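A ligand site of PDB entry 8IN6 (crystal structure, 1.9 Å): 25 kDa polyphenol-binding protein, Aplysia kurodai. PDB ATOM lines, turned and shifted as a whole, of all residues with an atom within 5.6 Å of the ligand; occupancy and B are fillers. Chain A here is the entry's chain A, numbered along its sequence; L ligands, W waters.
O of Gln 95 sits close to O7 of the ligand (3.4 Å). Residues that only touch the ligand: Pro 77, His 197 and Pro 201. Hydrophobic or aromatic side chains that line the ligand: Pro 77, Tyr 96, His 197, Met 198, Pro 199 and Pro 201. Within 4 Å of the ligand: Gly 74, Asn 75, Pro 77, Gln 95, Tyr 96, His 197, Met 198, Pro 199 and Pro 201.
Water W2 bridges the side-chain hydroxyl of Tyr 160 (2.7 Å) and an oxygen (O25) of the ligand (2.8 Å). Water W3 lies within hydrogen-bond range of an oxygen (O15) of the ligand (3.0 Å), the side-chain hydroxyl (OH) of Tyr 187 (3.0 Å) and the backbone carbonyl oxygen (O) of Pro 199 (3.3 Å). Water W1 lies within hydrogen-bond range of N of Val 158 and O24 of the ligand.
The backbone carbonyl oxygen (O) of Tyr 96 sits at hydrogen-bond distance from an oxygen (O14) of the ligand, 2.4 Å away. O4 of the ligand lies within hydrogen-bond range of OD1 of Asn 75. O10 of the ligand is in hydrogen-bond range of O of Gly 74. The backbone carbonyl oxygen (O) of Pro 199 lies within hydrogen-bond range of an oxygen (O16) of the ligand (3.1 Å). The side-chain sulfur of Met 198 sits close to an oxygen (O16) of the ligand, 3.7 Å away.
ND1 of His 197 lies within hydrogen-bond range of OH of Tyr 160 (3.4 Å). The backbone NH of Met 198 is in hydrogen-bond range of the backbone carbonyl oxygen of Tyr 187 (2.9 Å).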
ATOM      1  N   ALA A  72     -39.080  26.965  12.566  1.00  0.00           N
ATOM      2  CA  ALA A  72     -39.616  26.004  11.605  1.00  0.00           C
ATOM      3  C   ALA A  72     -39.343  24.593  12.111  1.00  0.00           C
ATOM      4  O   ALA A  72     -38.224  24.292  12.525  1.00  0.00           O
ATOM      5  CB  ALA A  72     -38.976  26.212  10.228  1.00  0.00           C
ATOM      6  N   TYR A  73     -40.374  23.744  12.109  1.00  0.00           N
ATOM      7  CA  TYR A  73     -40.247  22.483  12.825  1.00  0.00           C
ATOM      8  C   TYR A  73     -39.103  21.644  12.268  1.00  0.00           C
ATOM      9  O   TYR A  73     -38.481  20.881  13.025  1.00  0.00           O
ATOM     10  CB  TYR A  73     -41.576  21.711  12.815  1.00  0.00           C
ATOM     11  CG  TYR A  73     -41.989  21.125  11.483  1.00  0.00           C
ATOM     12  CD1 TYR A  73     -41.546  19.869  11.082  1.00  0.00           C
ATOM     13  CD2 TYR A  73     -42.862  21.821  10.651  1.00  0.00           C
ATOM     14  CE1 TYR A  73     -41.942  19.320   9.840  1.00  0.00           C
ATOM     15  CE2 TYR A  73     -43.250  21.295   9.410  1.00  0.00           C
ATOM     16  CZ  TYR A  73     -42.793  20.051   9.015  1.00  0.00           C
ATOM     17  OH  TYR A  73     -43.194  19.519   7.785  1.00  0.00           O
ATOM     18  N   GLY A  74     -38.752  21.833  10.989  1.00  0.00           N
ATOM     19  CA  GLY A  74     -37.652  21.079  10.406  1.00  0.00           C
ATOM     20  C   GLY A  74     -36.312  21.339  11.067  1.00  0.00           C
ATOM     21  O   GLY A  74     -35.407  20.494  11.010  1.00  0.00           O
ATOM     22  N   ASN A  75     -36.175  22.500  11.718  1.00  0.00           N
ATOM     23  CA  ASN A  75     -34.988  22.839  12.475  1.00  0.00           C
ATOM     24  C   ASN A  75     -34.944  22.203  13.857  1.00  0.00           C
ATOM     25  O   ASN A  75     -33.936  22.376  14.556  1.00  0.00           O
ATOM     26  CB  ASN A  75     -34.894  24.358  12.667  1.00  0.00           C
ATOM     27  CG  ASN A  75     -34.333  25.027  11.482  1.00  0.00           C
ATOM     28  OD1 ASN A  75     -33.537  24.444  10.749  1.00  0.00           O
ATOM     29  ND2 ASN A  75     -34.737  26.274  11.241  1.00  0.00           N
ATOM     30  N   VAL A  76     -36.018  21.550  14.293  1.00  0.00           N
ATOM     31  CA  VAL A  76     -36.075  21.035  15.651  1.00  0.00           C
ATOM     32  C   VAL A  76     -36.524  19.580  15.591  1.00  0.00           C
ATOM     33  O   VAL A  76     -37.681  19.267  15.924  1.00  0.00           O
ATOM     34  CB  VAL A  76     -37.020  21.863  16.546  1.00  0.00           C
ATOM     35  CG1 VAL A  76     -36.886  21.442  18.013  1.00  0.00           C
ATOM     36  CG2 VAL A  76     -36.710  23.346  16.425  1.00  0.00           C
ATOM     37  N   PRO A  77     -35.634  18.668  15.191  1.00  0.00           N
ATOM     38  CA  PRO A  77     -36.067  17.268  15.010  1.00  0.00           C
ATOM     39  C   PRO A  77     -36.453  16.594  16.304  1.00  0.00           C
ATOM     40  O   PRO A  77     -37.183  15.584  16.269  1.00  0.00           O
ATOM     41  CB  PRO A  77     -34.844  16.607  14.365  1.00  0.00           C
ATOM     42  CG  PRO A  77     -33.695  17.443  14.817  1.00  0.00           C
ATOM     43  CD  PRO A  77     -34.204  18.849  14.905  1.00  0.00           C
ATOM     44  N   GLN A  95     -28.795  11.553  17.112  1.00  0.00           N
ATOM     45  CA  GLN A  95     -29.369  12.523  16.182  1.00  0.00           C
ATOM     46  C   GLN A  95     -28.494  13.764  16.060  1.00  0.00           C
ATOM     47  O   GLN A  95     -28.414  14.369  14.977  1.00  0.00           O
ATOM     48  CB  GLN A  95     -30.766  12.927  16.630  1.00  0.00           C
ATOM     49  CG  GLN A  95     -31.912  12.088  16.070  1.00  0.00           C
ATOM     50  CD  GLN A  95     -33.186  12.887  15.936  1.00  0.00           C
ATOM     51  OE1 GLN A  95     -33.221  13.912  15.257  1.00  0.00           O
ATOM     52  NE2 GLN A  95     -34.238  12.443  16.613  1.00  0.00           N
ATOM     53  N   TYR A  96     -27.867  14.173  17.160  1.00  0.00           N
ATOM     54  CA  TYR A  96     -27.040  15.363  17.200  1.00  0.00           C
ATOM     55  C   TYR A  96     -25.555  15.069  17.373  1.00  0.00           C
ATOM     56  O   TYR A  96     -24.742  15.998  17.257  1.00  0.00           O
ATOM     57  CB  TYR A  96     -27.496  16.299  18.335  1.00  0.00           C
ATOM     58  CG  TYR A  96     -28.831  16.998  18.112  1.00  0.00           C
ATOM     59  CD1 TYR A  96     -29.356  17.170  16.825  1.00  0.00           C
ATOM     60  CD2 TYR A  96     -29.563  17.486  19.190  1.00  0.00           C
ATOM     61  CE1 TYR A  96     -30.580  17.826  16.646  1.00  0.00           C
ATOM     62  CE2 TYR A  96     -30.766  18.130  19.015  1.00  0.00           C
ATOM     63  CZ  TYR A  96     -31.274  18.304  17.750  1.00  0.00           C
ATOM     64  OH  TYR A  96     -32.480  18.951  17.612  1.00  0.00           O
ATOM     65  N   GLY A  97     -25.184  13.819  17.638  1.00  0.00           N
ATOM     66  CA  GLY A  97     -23.795  13.443  17.782  1.00  0.00           C
ATOM     67  C   GLY A  97     -23.162  13.964  19.054  1.00  0.00           C
ATOM     68  O   GLY A  97     -22.054  14.514  19.022  1.00  0.00           O
ATOM     69  N   VAL A 158     -25.631  33.702  11.983  1.00  0.00           N
ATOM     70  CA  VAL A 158     -24.339  34.265  12.350  1.00  0.00           C
ATOM     71  C   VAL A 158     -23.643  34.711  11.064  1.00  0.00           C
ATOM     72  O   VAL A 158     -23.402  33.899  10.165  1.00  0.00           O
ATOM     73  CB  VAL A 158     -23.477  33.263  13.116  1.00  0.00           C
ATOM     74  CG1 VAL A 158     -22.134  33.895  13.485  1.00  0.00           C
ATOM     75  CG2 VAL A 158     -24.209  32.737  14.346  1.00  0.00           C
ATOM     76  N   TYR A 160     -20.358  36.120   9.231  1.00  0.00           N
ATOM     77  CA  TYR A 160     -18.915  36.215   9.408  1.00  0.00           C
ATOM     78  C   TYR A 160     -18.373  37.319   8.521  1.00  0.00           C
ATOM     79  O   TYR A 160     -18.846  37.472   7.382  1.00  0.00           O
ATOM     80  CB  TYR A 160     -18.253  34.882   9.080  1.00  0.00           C
ATOM     81  CG  TYR A 160     -18.564  33.830  10.128  1.00  0.00           C
ATOM     82  CD1 TYR A 160     -19.723  33.045  10.047  1.00  0.00           C
ATOM     83  CD2 TYR A 160     -17.751  33.690  11.254  1.00  0.00           C
ATOM     84  CE1 TYR A 160     -20.037  32.117  11.053  1.00  0.00           C
ATOM     85  CE2 TYR A 160     -18.036  32.744  12.258  1.00  0.00           C
ATOM     86  CZ  TYR A 160     -19.198  31.975  12.152  1.00  0.00           C
ATOM     87  OH  TYR A 160     -19.490  31.075  13.149  1.00  0.00           O
ATOM     88  N   TYR A 187     -17.213  26.690  16.989  1.00  0.00           N
ATOM     89  CA  TYR A 187     -15.770  26.768  17.237  1.00  0.00           C
ATOM     90  C   TYR A 187     -15.003  26.951  15.926  1.00  0.00           C
ATOM     91  O   TYR A 187     -15.527  26.709  14.835  1.00  0.00           O
ATOM     92  CB  TYR A 187     -15.248  25.542  17.994  1.00  0.00           C
ATOM     93  CG  TYR A 187     -15.508  24.255  17.267  1.00  0.00           C
ATOM     94  CD1 TYR A 187     -16.709  23.566  17.448  1.00  0.00           C
ATOM     95  CD2 TYR A 187     -14.571  23.734  16.383  1.00  0.00           C
ATOM     96  CE1 TYR A 187     -16.954  22.364  16.783  1.00  0.00           C
ATOM     97  CE2 TYR A 187     -14.805  22.543  15.700  1.00  0.00           C
ATOM     98  CZ  TYR A 187     -16.002  21.867  15.912  1.00  0.00           C
ATOM     99  OH  TYR A 187     -16.226  20.694  15.238  1.00  0.00           O
ATOM    100  N   HIS A 197     -14.888  27.217  10.570  1.00  0.00           N
ATOM    101  CA  HIS A 197     -15.723  27.302  11.744  1.00  0.00           C
ATOM    102  C   HIS A 197     -16.830  26.290  11.580  1.00  0.00           C
ATOM    103  O   HIS A 197     -17.306  26.064  10.471  1.00  0.00           O
ATOM    104  CB  HIS A 197     -16.309  28.702  11.976  1.00  0.00           C
ATOM    105  CG  HIS A 197     -17.161  29.195  10.844  1.00  0.00           C
ATOM    106  ND1 HIS A 197     -18.499  28.885  10.738  1.00  0.00           N
ATOM    107  CD2 HIS A 197     -16.869  29.992   9.785  1.00  0.00           C
ATOM    108  CE1 HIS A 197     -18.996  29.460   9.657  1.00  0.00           C
ATOM    109  NE2 HIS A 197     -18.032  30.130   9.054  1.00  0.00           N
ATOM    110  N   MET A 198     -17.234  25.690  12.698  1.00  0.00           N
ATOM    111  CA  MET A 198     -18.191  24.619  12.684  1.00  0.00           C
ATOM    112  C   MET A 198     -19.084  24.720  13.908  1.00  0.00           C
ATOM    113  O   MET A 198     -18.593  25.015  15.011  1.00  0.00           O
ATOM    114  CB  MET A 198     -17.472  23.276  12.684  1.00  0.00           C
ATOM    115  CG  MET A 198     -18.104  22.261  11.771  1.00  0.00           C
ATOM    116  SD  MET A 198     -17.010  20.847  11.634  1.00  0.00           S
ATOM    117  CE  MET A 198     -16.528  21.035   9.908  1.00  0.00           C
ATOM    118  N   PRO A 199     -20.382  24.476  13.769  1.00  0.00           N
ATOM    119  CA  PRO A 199     -21.247  24.497  14.942  1.00  0.00           C
ATOM    120  C   PRO A 199     -20.913  23.337  15.851  1.00  0.00           C
ATOM    121  O   PRO A 199     -20.502  22.267  15.390  1.00  0.00           O
ATOM    122  CB  PRO A 199     -22.668  24.331  14.370  1.00  0.00           C
ATOM    123  CG  PRO A 199     -22.529  24.512  12.896  1.00  0.00           C
ATOM    124  CD  PRO A 199     -21.128  24.104  12.551  1.00  0.00           C
ATOM    125  N   CYS A 200     -21.079  23.564  17.140  1.00  0.00           N
ATOM    126  CA  CYS A 200     -21.174  22.473  18.085  1.00  0.00           C
ATOM    127  C   CYS A 200     -22.397  21.628  17.741  1.00  0.00           C
ATOM    128  O   CYS A 200     -23.333  22.113  17.092  1.00  0.00           O
ATOM    129  CB  CYS A 200     -21.309  23.022  19.495  1.00  0.00           C
ATOM    130  SG  CYS A 200     -19.789  23.700  20.179  1.00  0.00           S
ATOM    131  N   PRO A 201     -22.423  20.369  18.156  1.00  0.00           N
ATOM    132  CA  PRO A 201     -23.678  19.610  18.100  1.00  0.00           C
ATOM    133  C   PRO A 201     -24.828  20.433  18.671  1.00  0.00           C
ATOM    134  O   PRO A 201     -24.662  21.139  19.667  1.00  0.00           O
ATOM    135  CB  PRO A 201     -23.379  18.382  18.960  1.00  0.00           C
ATOM    136  CG  PRO A 201     -21.918  18.142  18.699  1.00  0.00           C
ATOM    137  CD  PRO A 201     -21.300  19.538  18.614  1.00  0.00           C
ATOM    138  N   ALA A 202     -25.993  20.368  18.018  1.00  0.00           N
ATOM    139  CA  ALA A 202     -27.095  21.220  18.438  1.00  0.00           C
ATOM    140  C   ALA A 202     -27.420  20.975  19.903  1.00  0.00           C
ATOM    141  O   ALA A 202     -27.424  19.830  20.373  1.00  0.00           O
ATOM    142  CB  ALA A 202     -28.334  20.978  17.580  1.00  0.00           C
HETATM  143  C1  LIG L   1     -28.381  20.953  11.888  1.00  0.00           C
HETATM  144  C2  LIG L   1     -26.986  21.585  11.737  1.00  0.00           C
HETATM  145  C3  LIG L   1     -26.623  22.047  10.387  1.00  0.00           C
HETATM  146  C4  LIG L   1     -27.736  22.147   9.394  1.00  0.00           C
HETATM  147  C5  LIG L   1     -28.759  20.994   9.513  1.00  0.00           C
HETATM  148  O1  LIG L   1     -28.674  20.159  10.712  1.00  0.00           O
HETATM  149  O2  LIG L   1     -30.142  21.425   9.483  1.00  0.00           O
HETATM  150  C6  LIG L   1     -30.917  20.315   9.041  1.00  0.00           C
HETATM  151  O3  LIG L   1     -30.479  19.223   8.974  1.00  0.00           O
HETATM  152  C7  LIG L   1     -32.379  20.578   8.625  1.00  0.00           C
HETATM  153  C8  LIG L   1     -32.858  21.882   8.742  1.00  0.00           C
HETATM  154  C9  LIG L   1     -34.188  22.164   8.361  1.00  0.00           C
HETATM  155  O4  LIG L   1     -34.724  23.491   8.474  1.00  0.00           O
HETATM  156  C10 LIG L   1     -34.969  21.141   7.855  1.00  0.00           C
HETATM  157  O5  LIG L   1     -36.285  21.405   7.473  1.00  0.00           O
HETATM  158  C11 LIG L   1     -34.469  19.831   7.732  1.00  0.00           C
HETATM  159  O6  LIG L   1     -35.331  18.806   7.197  1.00  0.00           O
HETATM  160  C12 LIG L   1     -33.153  19.531   8.116  1.00  0.00           C
HETATM  161  C13 LIG L   1     -29.638  17.868  12.903  1.00  0.00           C
HETATM  162  O7  LIG L   1     -28.690  17.225  13.221  1.00  0.00           O
HETATM  163  C14 LIG L   1     -30.859  17.165  12.222  1.00  0.00           C
HETATM  164  C15 LIG L   1     -30.859  15.765  12.093  1.00  0.00           C
HETATM  165  C16 LIG L   1     -31.934  15.137  11.502  1.00  0.00           C
HETATM  166  O8  LIG L   1     -31.950  13.714  11.360  1.00  0.00           O
HETATM  167  C17 LIG L   1     -33.032  15.879  11.024  1.00  0.00           C
HETATM  168  O9  LIG L   1     -34.123  15.228  10.419  1.00  0.00           O
HETATM  169  C18 LIG L   1     -33.047  17.267  11.146  1.00  0.00           C
HETATM  170  O10 LIG L   1     -34.173  17.970  10.682  1.00  0.00           O
HETATM  171  C19 LIG L   1     -31.971  17.907  11.745  1.00  0.00           C
HETATM  172  C20 LIG L   1     -28.408  19.972  13.127  1.00  0.00           C
HETATM  173  O11 LIG L   1     -29.671  19.302  13.184  1.00  0.00           O
HETATM  174  O12 LIG L   1     -26.028  20.555  12.137  1.00  0.00           O
HETATM  175  C21 LIG L   1     -25.017  21.089  13.017  1.00  0.00           C
HETATM  176  O13 LIG L   1     -25.081  22.201  13.389  1.00  0.00           O
HETATM  177  C22 LIG L   1     -23.869  20.192  13.515  1.00  0.00           C
HETATM  178  C23 LIG L   1     -24.166  19.097  14.301  1.00  0.00           C
HETATM  179  C24 LIG L   1     -23.134  18.274  14.772  1.00  0.00           C
HETATM  180  O14 LIG L   1     -23.414  17.128  15.584  1.00  0.00           O
HETATM  181  C25 LIG L   1     -21.811  18.575  14.451  1.00  0.00           C
HETATM  182  O15 LIG L   1     -20.826  17.731  14.949  1.00  0.00           O
HETATM  183  C26 LIG L   1     -21.515  19.675  13.657  1.00  0.00           C
HETATM  184  O16 LIG L   1     -20.189  20.003  13.305  1.00  0.00           O
HETATM  185  C27 LIG L   1     -22.554  20.487  13.191  1.00  0.00           C
HETATM  186  O17 LIG L   1     -28.315  23.424   9.446  1.00  0.00           O
HETATM  187  C28 LIG L   1     -28.650  24.043   8.199  1.00  0.00           C
HETATM  188  O18 LIG L   1     -29.796  24.338   8.007  1.00  0.00           O
HETATM  189  C29 LIG L   1     -27.633  24.446   7.068  1.00  0.00           C
HETATM  190  C30 LIG L   1     -27.319  25.790   6.945  1.00  0.00           C
HETATM  191  C31 LIG L   1     -26.423  26.238   5.934  1.00  0.00           C
HETATM  192  O19 LIG L   1     -26.117  27.602   5.860  1.00  0.00           O
HETATM  193  C32 LIG L   1     -25.863  25.325   5.038  1.00  0.00           C
HETATM  194  O20 LIG L   1     -24.960  25.802   4.020  1.00  0.00           O
HETATM  195  C33 LIG L   1     -26.194  23.963   5.139  1.00  0.00           C
HETATM  196  O21 LIG L   1     -25.650  23.027   4.230  1.00  0.00           O
HETATM  197  C34 LIG L   1     -27.090  23.515   6.150  1.00  0.00           C
HETATM  198  O22 LIG L   1     -26.060  23.346  10.541  1.00  0.00           O
HETATM  199  C35 LIG L   1     -24.867  23.656   9.805  1.00  0.00           C
HETATM  200  O23 LIG L   1     -24.327  22.892   9.106  1.00  0.00           O
HETATM  201  C36 LIG L   1     -24.288  25.088  10.026  1.00  0.00           C
HETATM  202  C37 LIG L   1     -25.085  26.025  10.691  1.00  0.00           C
HETATM  203  C38 LIG L   1     -24.600  27.306  10.912  1.00  0.00           C
HETATM  204  O24 LIG L   1     -25.446  28.216  11.588  1.00  0.00           O
HETATM  205  C39 LIG L   1     -23.317  27.657  10.485  1.00  0.00           C
HETATM  206  O25 LIG L   1     -22.819  28.939  10.706  1.00  0.00           O
HETATM  207  C40 LIG L   1     -22.513  26.709   9.825  1.00  0.00           C
HETATM  208  O26 LIG L   1     -21.226  27.017   9.372  1.00  0.00           O
HETATM  209  C41 LIG L   1     -23.012  25.416   9.598  1.00  0.00           C
HETATM  210  O   HOH W   1     -26.232  31.139  11.726  1.00  0.00           O
HETATM  211  O   HOH W   2     -21.879  29.732  13.225  1.00  0.00           O
HETATM  212  O   HOH W   3     -18.835  19.522  16.235  1.00  0.00           O
